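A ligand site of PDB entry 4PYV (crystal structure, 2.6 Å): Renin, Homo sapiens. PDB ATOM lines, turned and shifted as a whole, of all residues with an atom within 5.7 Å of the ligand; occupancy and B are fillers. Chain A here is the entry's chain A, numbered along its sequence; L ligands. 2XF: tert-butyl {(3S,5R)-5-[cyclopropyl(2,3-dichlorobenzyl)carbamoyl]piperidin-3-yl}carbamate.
A nitrogen (N3) of the ligand is in salt-bridge range of the side-chain carboxylate (OD1) of Asp 38.
The side-chain carboxylate (OD2) of Asp 226 is in salt-bridge range of a nitrogen (N3) of the ligand.
The side-chain hydroxyl of Thr 85 lies within hydrogen-bond range of an oxygen (O9) of the ligand (3.2 Å).
The side-chain hydroxyl (OG) of Ser 41 sits at hydrogen-bond distance from the side-chain carboxylate (OD2) of Asp 38 (2.8 Å).
OD1 of Asp 38 is in hydrogen-bond range of N of Gly 40 (3.1 Å).
The backbone NH of Gly 228 sits close to the side-chain carboxylate of Asp 226, at 3.2 Å.
The backbone NH (N) of Gly 40 lies within hydrogen-bond range of the side-chain carboxylate (OD1) of Asp 226 (3.2 Å).
OG of Ser 230 sits at hydrogen-bond distance from O of Thr 18, 2.7 Å away.
NE2 of Gln 19 sits at hydrogen-bond distance from O of Leu 121, 3.0 Å away.
Gln 19 touches the ligand (CG to C18, 3.9 Å).
CG1 of Val 36 touches C14 of the ligand, 3.6 Å away.
O of Gly 40 touches C2 of the ligand (3.5 Å).
CB of Ser 41 touches O24 of the ligand, 3.2 Å away.
Arg 82 touches the ligand (O to C27, 3.5 Å).
Tyr 83 touches the ligand (CE1 to O24, 3.1 Å).
Ser 84 touches the ligand (OG to C6, 3.9 Å).
O of Pro 118 touches CL2 of the ligand, at 3.7 Å.
CE1 of Phe 119 touches CL1 of the ligand, at 3.7 Å.
N of Ala 122 touches CL2 of the ligand (3.8 Å).
Phe 124 touches the ligand (CZ to C13, 3.7 Å).
CG2 of Val 127 touches C13 of the ligand, at 3.7 Å.
Gly 228 touches the ligand.
Ala 229 touches the ligand (N to C4, 3.7 Å).
Ser 230 touches the ligand (OG to C17, 3.3 Å).
Within 4 Å of the ligand: Gln 19, Val 36, Asp 38, Gly 40, Ser 41, Arg 82, Tyr 83, Ser 84, Thr 85, Pro 118, Phe 119, Ala 122, Phe 124, Val 127, Asp 226, Gly 228, Ala 229 and Ser 230.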
ATOM      1  N   THR A  18      38.234 -21.878   0.555  1.00  0.00           N
ATOM      2  CA  THR A  18      36.841 -22.258   0.347  1.00  0.00           C
ATOM      3  C   THR A  18      36.542 -23.653   0.830  1.00  0.00           C
ATOM      4  O   THR A  18      35.393 -23.932   1.156  1.00  0.00           O
ATOM      5  CB  THR A  18      36.450 -22.096  -1.126  1.00  0.00           C
ATOM      6  OG1 THR A  18      37.360 -22.823  -1.938  1.00  0.00           O
ATOM      7  CG2 THR A  18      36.421 -20.676  -1.567  1.00  0.00           C
ATOM      8  N   GLN A  19      37.542 -24.562   0.823  1.00  0.00           N
ATOM      9  CA  GLN A  19      37.268 -25.924   1.297  1.00  0.00           C
ATOM     10  C   GLN A  19      38.310 -26.294   2.286  1.00  0.00           C
ATOM     11  O   GLN A  19      39.505 -26.155   1.996  1.00  0.00           O
ATOM     12  CB  GLN A  19      37.263 -26.948   0.157  1.00  0.00           C
ATOM     13  CG  GLN A  19      36.148 -26.749  -0.876  1.00  0.00           C
ATOM     14  CD  GLN A  19      36.441 -27.419  -2.182  1.00  0.00           C
ATOM     15  OE1 GLN A  19      36.993 -28.532  -2.211  1.00  0.00           O
ATOM     16  NE2 GLN A  19      36.042 -26.772  -3.285  1.00  0.00           N
ATOM     17  N   VAL A  36      34.693 -32.875   4.569  1.00  0.00           N
ATOM     18  CA  VAL A  36      34.366 -31.580   5.153  1.00  0.00           C
ATOM     19  C   VAL A  36      33.568 -31.847   6.463  1.00  0.00           C
ATOM     20  O   VAL A  36      32.619 -32.618   6.440  1.00  0.00           O
ATOM     21  CB  VAL A  36      33.549 -30.740   4.135  1.00  0.00           C
ATOM     22  CG1 VAL A  36      32.889 -29.567   4.826  1.00  0.00           C
ATOM     23  CG2 VAL A  36      34.428 -30.273   2.997  1.00  0.00           C
ATOM     24  N   ASP A  38      31.037 -30.469   8.684  1.00  0.00           N
ATOM     25  CA  ASP A  38      29.909 -29.555   8.492  1.00  0.00           C
ATOM     26  C   ASP A  38      28.946 -29.399   9.696  1.00  0.00           C
ATOM     27  O   ASP A  38      28.183 -30.308   9.972  1.00  0.00           O
ATOM     28  CB  ASP A  38      29.139 -30.028   7.241  1.00  0.00           C
ATOM     29  CG  ASP A  38      27.998 -29.190   6.695  1.00  0.00           C
ATOM     30  OD1 ASP A  38      27.881 -28.022   7.103  1.00  0.00           O
ATOM     31  OD2 ASP A  38      27.280 -29.677   5.796  1.00  0.00           O
ATOM     32  N   GLY A  40      26.431 -27.335   9.714  1.00  0.00           N
ATOM     33  CA  GLY A  40      25.128 -27.077   9.112  1.00  0.00           C
ATOM     34  C   GLY A  40      24.350 -28.304   8.650  1.00  0.00           C
ATOM     35  O   GLY A  40      23.278 -28.144   8.068  1.00  0.00           O
ATOM     36  N   SER A  41      24.888 -29.524   8.863  1.00  0.00           N
ATOM     37  CA  SER A  41      24.286 -30.820   8.487  1.00  0.00           C
ATOM     38  C   SER A  41      24.670 -31.902   9.504  1.00  0.00           C
ATOM     39  O   SER A  41      25.593 -31.684  10.285  1.00  0.00           O
ATOM     40  CB  SER A  41      24.655 -31.231   7.062  1.00  0.00           C
ATOM     41  OG  SER A  41      25.943 -31.812   6.975  1.00  0.00           O
ATOM     42  N   LEU A  81      19.643 -36.201   0.137  1.00  0.00           N
ATOM     43  CA  LEU A  81      20.162 -35.025   0.823  1.00  0.00           C
ATOM     44  C   LEU A  81      20.061 -33.869  -0.129  1.00  0.00           C
ATOM     45  O   LEU A  81      20.740 -33.840  -1.162  1.00  0.00           O
ATOM     46  CB  LEU A  81      21.623 -35.262   1.263  1.00  0.00           C
ATOM     47  CG  LEU A  81      21.911 -36.557   2.025  1.00  0.00           C
ATOM     48  CD1 LEU A  81      23.397 -36.744   2.194  1.00  0.00           C
ATOM     49  CD2 LEU A  81      21.260 -36.548   3.389  1.00  0.00           C
ATOM     50  N   ARG A  82      19.156 -32.938   0.171  1.00  0.00           N
ATOM     51  CA  ARG A  82      18.961 -31.762  -0.671  1.00  0.00           C
ATOM     52  C   ARG A  82      19.724 -30.631  -0.051  1.00  0.00           C
ATOM     53  O   ARG A  82      19.370 -30.150   1.026  1.00  0.00           O
ATOM     54  CB  ARG A  82      17.469 -31.440  -0.891  1.00  0.00           C
ATOM     55  CG  ARG A  82      16.794 -32.375  -1.899  1.00  0.00           C
ATOM     56  CD  ARG A  82      15.282 -32.442  -1.703  1.00  0.00           C
ATOM     57  NE  ARG A  82      14.703 -33.631  -2.337  1.00  0.00           N
ATOM     58  CZ  ARG A  82      14.307 -34.719  -1.677  1.00  0.00           C
ATOM     59  NH1 ARG A  82      14.402 -34.771  -0.356  1.00  0.00           N
ATOM     60  NH2 ARG A  82      13.814 -35.762  -2.344  1.00  0.00           N
ATOM     61  N   TYR A  83      20.847 -30.311  -0.660  1.00  0.00           N
ATOM     62  CA  TYR A  83      21.737 -29.255  -0.199  1.00  0.00           C
ATOM     63  C   TYR A  83      21.361 -27.948  -0.902  1.00  0.00           C
ATOM     64  O   TYR A  83      20.783 -27.963  -1.990  1.00  0.00           O
ATOM     65  CB  TYR A  83      23.231 -29.643  -0.488  1.00  0.00           C
ATOM     66  CG  TYR A  83      23.808 -30.692   0.450  1.00  0.00           C
ATOM     67  CD1 TYR A  83      24.045 -30.404   1.789  1.00  0.00           C
ATOM     68  CD2 TYR A  83      24.164 -31.953  -0.015  1.00  0.00           C
ATOM     69  CE1 TYR A  83      24.590 -31.358   2.650  1.00  0.00           C
ATOM     70  CE2 TYR A  83      24.707 -32.914   0.839  1.00  0.00           C
ATOM     71  CZ  TYR A  83      24.927 -32.603   2.171  1.00  0.00           C
ATOM     72  OH  TYR A  83      25.449 -33.503   3.067  1.00  0.00           O
ATOM     73  N   SER A  84      21.702 -26.816  -0.258  1.00  0.00           N
ATOM     74  CA  SER A  84      21.468 -25.474  -0.804  1.00  0.00           C
ATOM     75  C   SER A  84      22.260 -25.249  -2.112  1.00  0.00           C
ATOM     76  O   SER A  84      21.851 -24.432  -2.942  1.00  0.00           O
ATOM     77  CB  SER A  84      21.787 -24.396   0.231  1.00  0.00           C
ATOM     78  OG  SER A  84      23.083 -24.526   0.789  1.00  0.00           O
ATOM     79  N   THR A  85      23.393 -25.998  -2.290  1.00  0.00           N
ATOM     80  CA  THR A  85      24.298 -25.983  -3.445  1.00  0.00           C
ATOM     81  C   THR A  85      23.965 -27.087  -4.493  1.00  0.00           C
ATOM     82  O   THR A  85      24.321 -26.930  -5.663  1.00  0.00           O
ATOM     83  CB  THR A  85      25.779 -26.051  -2.994  1.00  0.00           C
ATOM     84  OG1 THR A  85      25.899 -26.928  -1.883  1.00  0.00           O
ATOM     85  CG2 THR A  85      26.368 -24.690  -2.639  1.00  0.00           C
ATOM     86  N   PRO A 118      27.604 -29.367  -8.389  1.00  0.00           N
ATOM     87  CA  PRO A 118      28.891 -28.771  -7.940  1.00  0.00           C
ATOM     88  C   PRO A 118      30.065 -29.701  -7.564  1.00  0.00           C
ATOM     89  O   PRO A 118      31.173 -29.201  -7.304  1.00  0.00           O
ATOM     90  CB  PRO A 118      28.456 -28.020  -6.665  1.00  0.00           C
ATOM     91  CG  PRO A 118      27.430 -28.957  -6.059  1.00  0.00           C
ATOM     92  CD  PRO A 118      26.696 -29.574  -7.239  1.00  0.00           C
ATOM     93  N   PHE A 119      29.831 -31.018  -7.488  1.00  0.00           N
ATOM     94  CA  PHE A 119      30.817 -31.959  -6.971  1.00  0.00           C
ATOM     95  C   PHE A 119      32.058 -32.164  -7.868  1.00  0.00           C
ATOM     96  O   PHE A 119      33.015 -32.746  -7.382  1.00  0.00           O
ATOM     97  CB  PHE A 119      30.152 -33.276  -6.566  1.00  0.00           C
ATOM     98  CG  PHE A 119      29.251 -33.027  -5.365  1.00  0.00           C
ATOM     99  CD1 PHE A 119      29.785 -32.847  -4.094  1.00  0.00           C
ATOM    100  CD2 PHE A 119      27.875 -32.846  -5.532  1.00  0.00           C
ATOM    101  CE1 PHE A 119      28.947 -32.536  -3.010  1.00  0.00           C
ATOM    102  CE2 PHE A 119      27.059 -32.516  -4.441  1.00  0.00           C
ATOM    103  CZ  PHE A 119      27.599 -32.366  -3.198  1.00  0.00           C
ATOM    104  N   LEU A 121      33.864 -29.654  -8.511  1.00  0.00           N
ATOM    105  CA  LEU A 121      34.669 -28.585  -7.906  1.00  0.00           C
ATOM    106  C   LEU A 121      35.151 -28.967  -6.526  1.00  0.00           C
ATOM    107  O   LEU A 121      35.982 -28.271  -5.932  1.00  0.00           O
ATOM    108  CB  LEU A 121      33.882 -27.272  -7.799  1.00  0.00           C
ATOM    109  CG  LEU A 121      33.267 -26.681  -9.098  1.00  0.00           C
ATOM    110  CD1 LEU A 121      32.370 -25.516  -8.780  1.00  0.00           C
ATOM    111  CD2 LEU A 121      34.334 -26.277 -10.116  1.00  0.00           C
ATOM    112  N   ALA A 122      34.581 -30.043  -5.966  1.00  0.00           N
ATOM    113  CA  ALA A 122      34.929 -30.523  -4.622  1.00  0.00           C
ATOM    114  C   ALA A 122      36.281 -31.261  -4.645  1.00  0.00           C
ATOM    115  O   ALA A 122      36.506 -32.149  -5.471  1.00  0.00           O
ATOM    116  CB  ALA A 122      33.833 -31.438  -4.084  1.00  0.00           C
ATOM    117  N   PHE A 124      37.290 -32.454  -1.741  1.00  0.00           N
ATOM    118  CA  PHE A 124      36.917 -33.453  -0.743  1.00  0.00           C
ATOM    119  C   PHE A 124      36.027 -34.542  -1.387  1.00  0.00           C
ATOM    120  O   PHE A 124      35.374 -34.276  -2.404  1.00  0.00           O
ATOM    121  CB  PHE A 124      36.168 -32.767   0.432  1.00  0.00           C
ATOM    122  CG  PHE A 124      34.915 -31.992   0.055  1.00  0.00           C
ATOM    123  CD1 PHE A 124      34.996 -30.670  -0.348  1.00  0.00           C
ATOM    124  CD2 PHE A 124      33.667 -32.591   0.120  1.00  0.00           C
ATOM    125  CE1 PHE A 124      33.839 -29.955  -0.692  1.00  0.00           C
ATOM    126  CE2 PHE A 124      32.509 -31.876  -0.239  1.00  0.00           C
ATOM    127  CZ  PHE A 124      32.608 -30.570  -0.642  1.00  0.00           C
ATOM    128  N   VAL A 127      31.226 -35.777   3.331  1.00  0.00           N
ATOM    129  CA  VAL A 127      30.913 -34.866   4.422  1.00  0.00           C
ATOM    130  C   VAL A 127      30.665 -35.597   5.729  1.00  0.00           C
ATOM    131  O   VAL A 127      30.039 -36.627   5.733  1.00  0.00           O
ATOM    132  CB  VAL A 127      29.676 -33.951   4.028  1.00  0.00           C
ATOM    133  CG1 VAL A 127      29.345 -32.938   5.118  1.00  0.00           C
ATOM    134  CG2 VAL A 127      29.857 -33.256   2.667  1.00  0.00           C
ATOM    135  N   GLN A 135      18.376 -32.738  12.713  1.00  0.00           N
ATOM    136  CA  GLN A 135      18.584 -32.389  11.299  1.00  0.00           C
ATOM    137  C   GLN A 135      19.055 -33.585  10.460  1.00  0.00           C
ATOM    138  O   GLN A 135      19.205 -33.446   9.242  1.00  0.00           O
ATOM    139  CB  GLN A 135      19.592 -31.236  11.123  1.00  0.00           C
ATOM    140  CG  GLN A 135      19.358 -30.005  11.973  1.00  0.00           C
ATOM    141  CD  GLN A 135      19.680 -28.746  11.208  1.00  0.00           C
ATOM    142  OE1 GLN A 135      18.800 -28.205  10.521  1.00  0.00           O
ATOM    143  NE2 GLN A 135      20.913 -28.235  11.307  1.00  0.00           N
ATOM    144  N   ILE A 137      18.888 -36.651   8.284  1.00  0.00           N
ATOM    145  CA  ILE A 137      17.999 -37.276   7.309  1.00  0.00           C
ATOM    146  C   ILE A 137      17.946 -38.752   7.606  1.00  0.00           C
ATOM    147  O   ILE A 137      18.994 -39.394   7.749  1.00  0.00           O
ATOM    148  CB  ILE A 137      18.476 -36.951   5.877  1.00  0.00           C
ATOM    149  CG1 ILE A 137      18.601 -35.404   5.640  1.00  0.00           C
ATOM    150  CG2 ILE A 137      17.626 -37.646   4.795  1.00  0.00           C
ATOM    151  CD1 ILE A 137      17.313 -34.577   5.490  1.00  0.00           C
ATOM    152  N   LEU A 224      23.334 -18.831  11.612  1.00  0.00           N
ATOM    153  CA  LEU A 224      23.742 -20.225  11.606  1.00  0.00           C
ATOM    154  C   LEU A 224      25.278 -20.245  11.509  1.00  0.00           C
ATOM    155  O   LEU A 224      25.851 -19.623  10.608  1.00  0.00           O
ATOM    156  CB  LEU A 224      23.085 -20.952  10.397  1.00  0.00           C
ATOM    157  CG  LEU A 224      23.514 -22.411  10.094  1.00  0.00           C
ATOM    158  CD1 LEU A 224      22.994 -23.399  11.133  1.00  0.00           C
ATOM    159  CD2 LEU A 224      23.090 -22.813   8.701  1.00  0.00           C
ATOM    160  N   ASP A 226      28.012 -22.181  10.490  1.00  0.00           N
ATOM    161  CA  ASP A 226      28.220 -23.249   9.519  1.00  0.00           C
ATOM    162  C   ASP A 226      29.659 -23.442   9.024  1.00  0.00           C
ATOM    163  O   ASP A 226      30.100 -22.806   8.057  1.00  0.00           O
ATOM    164  CB  ASP A 226      27.278 -22.980   8.329  1.00  0.00           C
ATOM    165  CG  ASP A 226      26.964 -24.148   7.444  1.00  0.00           C
ATOM    166  OD1 ASP A 226      27.550 -25.225   7.660  1.00  0.00           O
ATOM    167  OD2 ASP A 226      26.152 -23.983   6.526  1.00  0.00           O
ATOM    168  N   GLY A 228      30.687 -25.844   7.287  1.00  0.00           N
ATOM    169  CA  GLY A 228      30.608 -26.407   5.946  1.00  0.00           C
ATOM    170  C   GLY A 228      30.363 -25.394   4.846  1.00  0.00           C
ATOM    171  O   GLY A 228      30.450 -25.724   3.671  1.00  0.00           O
ATOM    172  N   ALA A 229      30.011 -24.163   5.226  1.00  0.00           N
ATOM    173  CA  ALA A 229      29.765 -23.111   4.246  1.00  0.00           C
ATOM    174  C   ALA A 229      31.093 -22.369   3.991  1.00  0.00           C
ATOM    175  O   ALA A 229      31.804 -22.051   4.964  1.00  0.00           O
ATOM    176  CB  ALA A 229      28.678 -22.169   4.766  1.00  0.00           C
ATOM    177  N   SER A 230      31.474 -22.144   2.721  1.00  0.00           N
ATOM    178  CA  SER A 230      32.721 -21.451   2.343  1.00  0.00           C
ATOM    179  C   SER A 230      32.681 -19.965   2.743  1.00  0.00           C
ATOM    180  O   SER A 230      33.645 -19.414   3.291  1.00  0.00           O
ATOM    181  CB  SER A 230      32.938 -21.503   0.834  1.00  0.00           C
ATOM    182  OG  SER A 230      33.034 -22.813   0.302  1.00  0.00           O
HETATM  183  C1  2XF L   1      24.513 -27.577   4.133  1.00  0.00           C
HETATM  184  C2  2XF L   1      24.985 -26.707   5.327  1.00  0.00           C
HETATM  185  N3  2XF L   1      26.455 -26.468   5.321  1.00  0.00           N
HETATM  186  C4  2XF L   1      27.099 -26.054   4.044  1.00  0.00           C
HETATM  187  C5  2XF L   1      26.784 -27.188   3.038  1.00  0.00           C
HETATM  188  C6  2XF L   1      25.229 -27.143   2.824  1.00  0.00           C
HETATM  189  C7  2XF L   1      27.514 -27.142   1.692  1.00  0.00           C
HETATM  190  N8  2XF L   1      28.412 -28.075   1.222  1.00  0.00           N
HETATM  191  O9  2XF L   1      27.172 -26.217   0.972  1.00  0.00           O
HETATM  192  N10 2XF L   1      23.035 -27.603   4.051  1.00  0.00           N
HETATM  193  C11 2XF L   1      28.824 -29.271   1.992  1.00  0.00           C
HETATM  194  C12 2XF L   1      28.790 -27.995  -0.189  1.00  0.00           C
HETATM  195  C13 2XF L   1      30.327 -29.619   2.049  1.00  0.00           C
HETATM  196  C14 2XF L   1      29.622 -29.086   3.302  1.00  0.00           C
HETATM  197  C15 2XF L   1      30.088 -27.346  -0.688  1.00  0.00           C
HETATM  198  C16 2XF L   1      30.770 -26.332   0.007  1.00  0.00           C
HETATM  199  C17 2XF L   1      31.914 -25.751  -0.584  1.00  0.00           C
HETATM  200  C18 2XF L   1      32.382 -26.150  -1.851  1.00  0.00           C
HETATM  201  C19 2XF L   1      31.673 -27.132  -2.559  1.00  0.00           C
HETATM  202  C20 2XF L   1      30.528 -27.713  -1.982  1.00  0.00           C
HETATM  203 CL1  2XF L   1      29.662 -28.930  -2.901  1.00  0.00          CL
HETATM  204 CL2  2XF L   1      32.188 -27.620  -4.173  1.00  0.00          CL
HETATM  205  C23 2XF L   1      22.409 -28.754   4.424  1.00  0.00           C
HETATM  206  O24 2XF L   1      23.028 -29.761   4.766  1.00  0.00           O
HETATM  207  O25 2XF L   1      21.063 -28.702   4.385  1.00  0.00           O
HETATM  208  C26 2XF L   1      20.201 -29.818   4.817  1.00  0.00           C
HETATM  209  C27 2XF L   1      20.501 -31.239   4.179  1.00  0.00           C
HETATM  210  C28 2XF L   1      20.341 -29.907   6.369  1.00  0.00           C
HETATM  211  C29 2XF L   1      18.707 -29.490   4.519  1.00  0.00           C
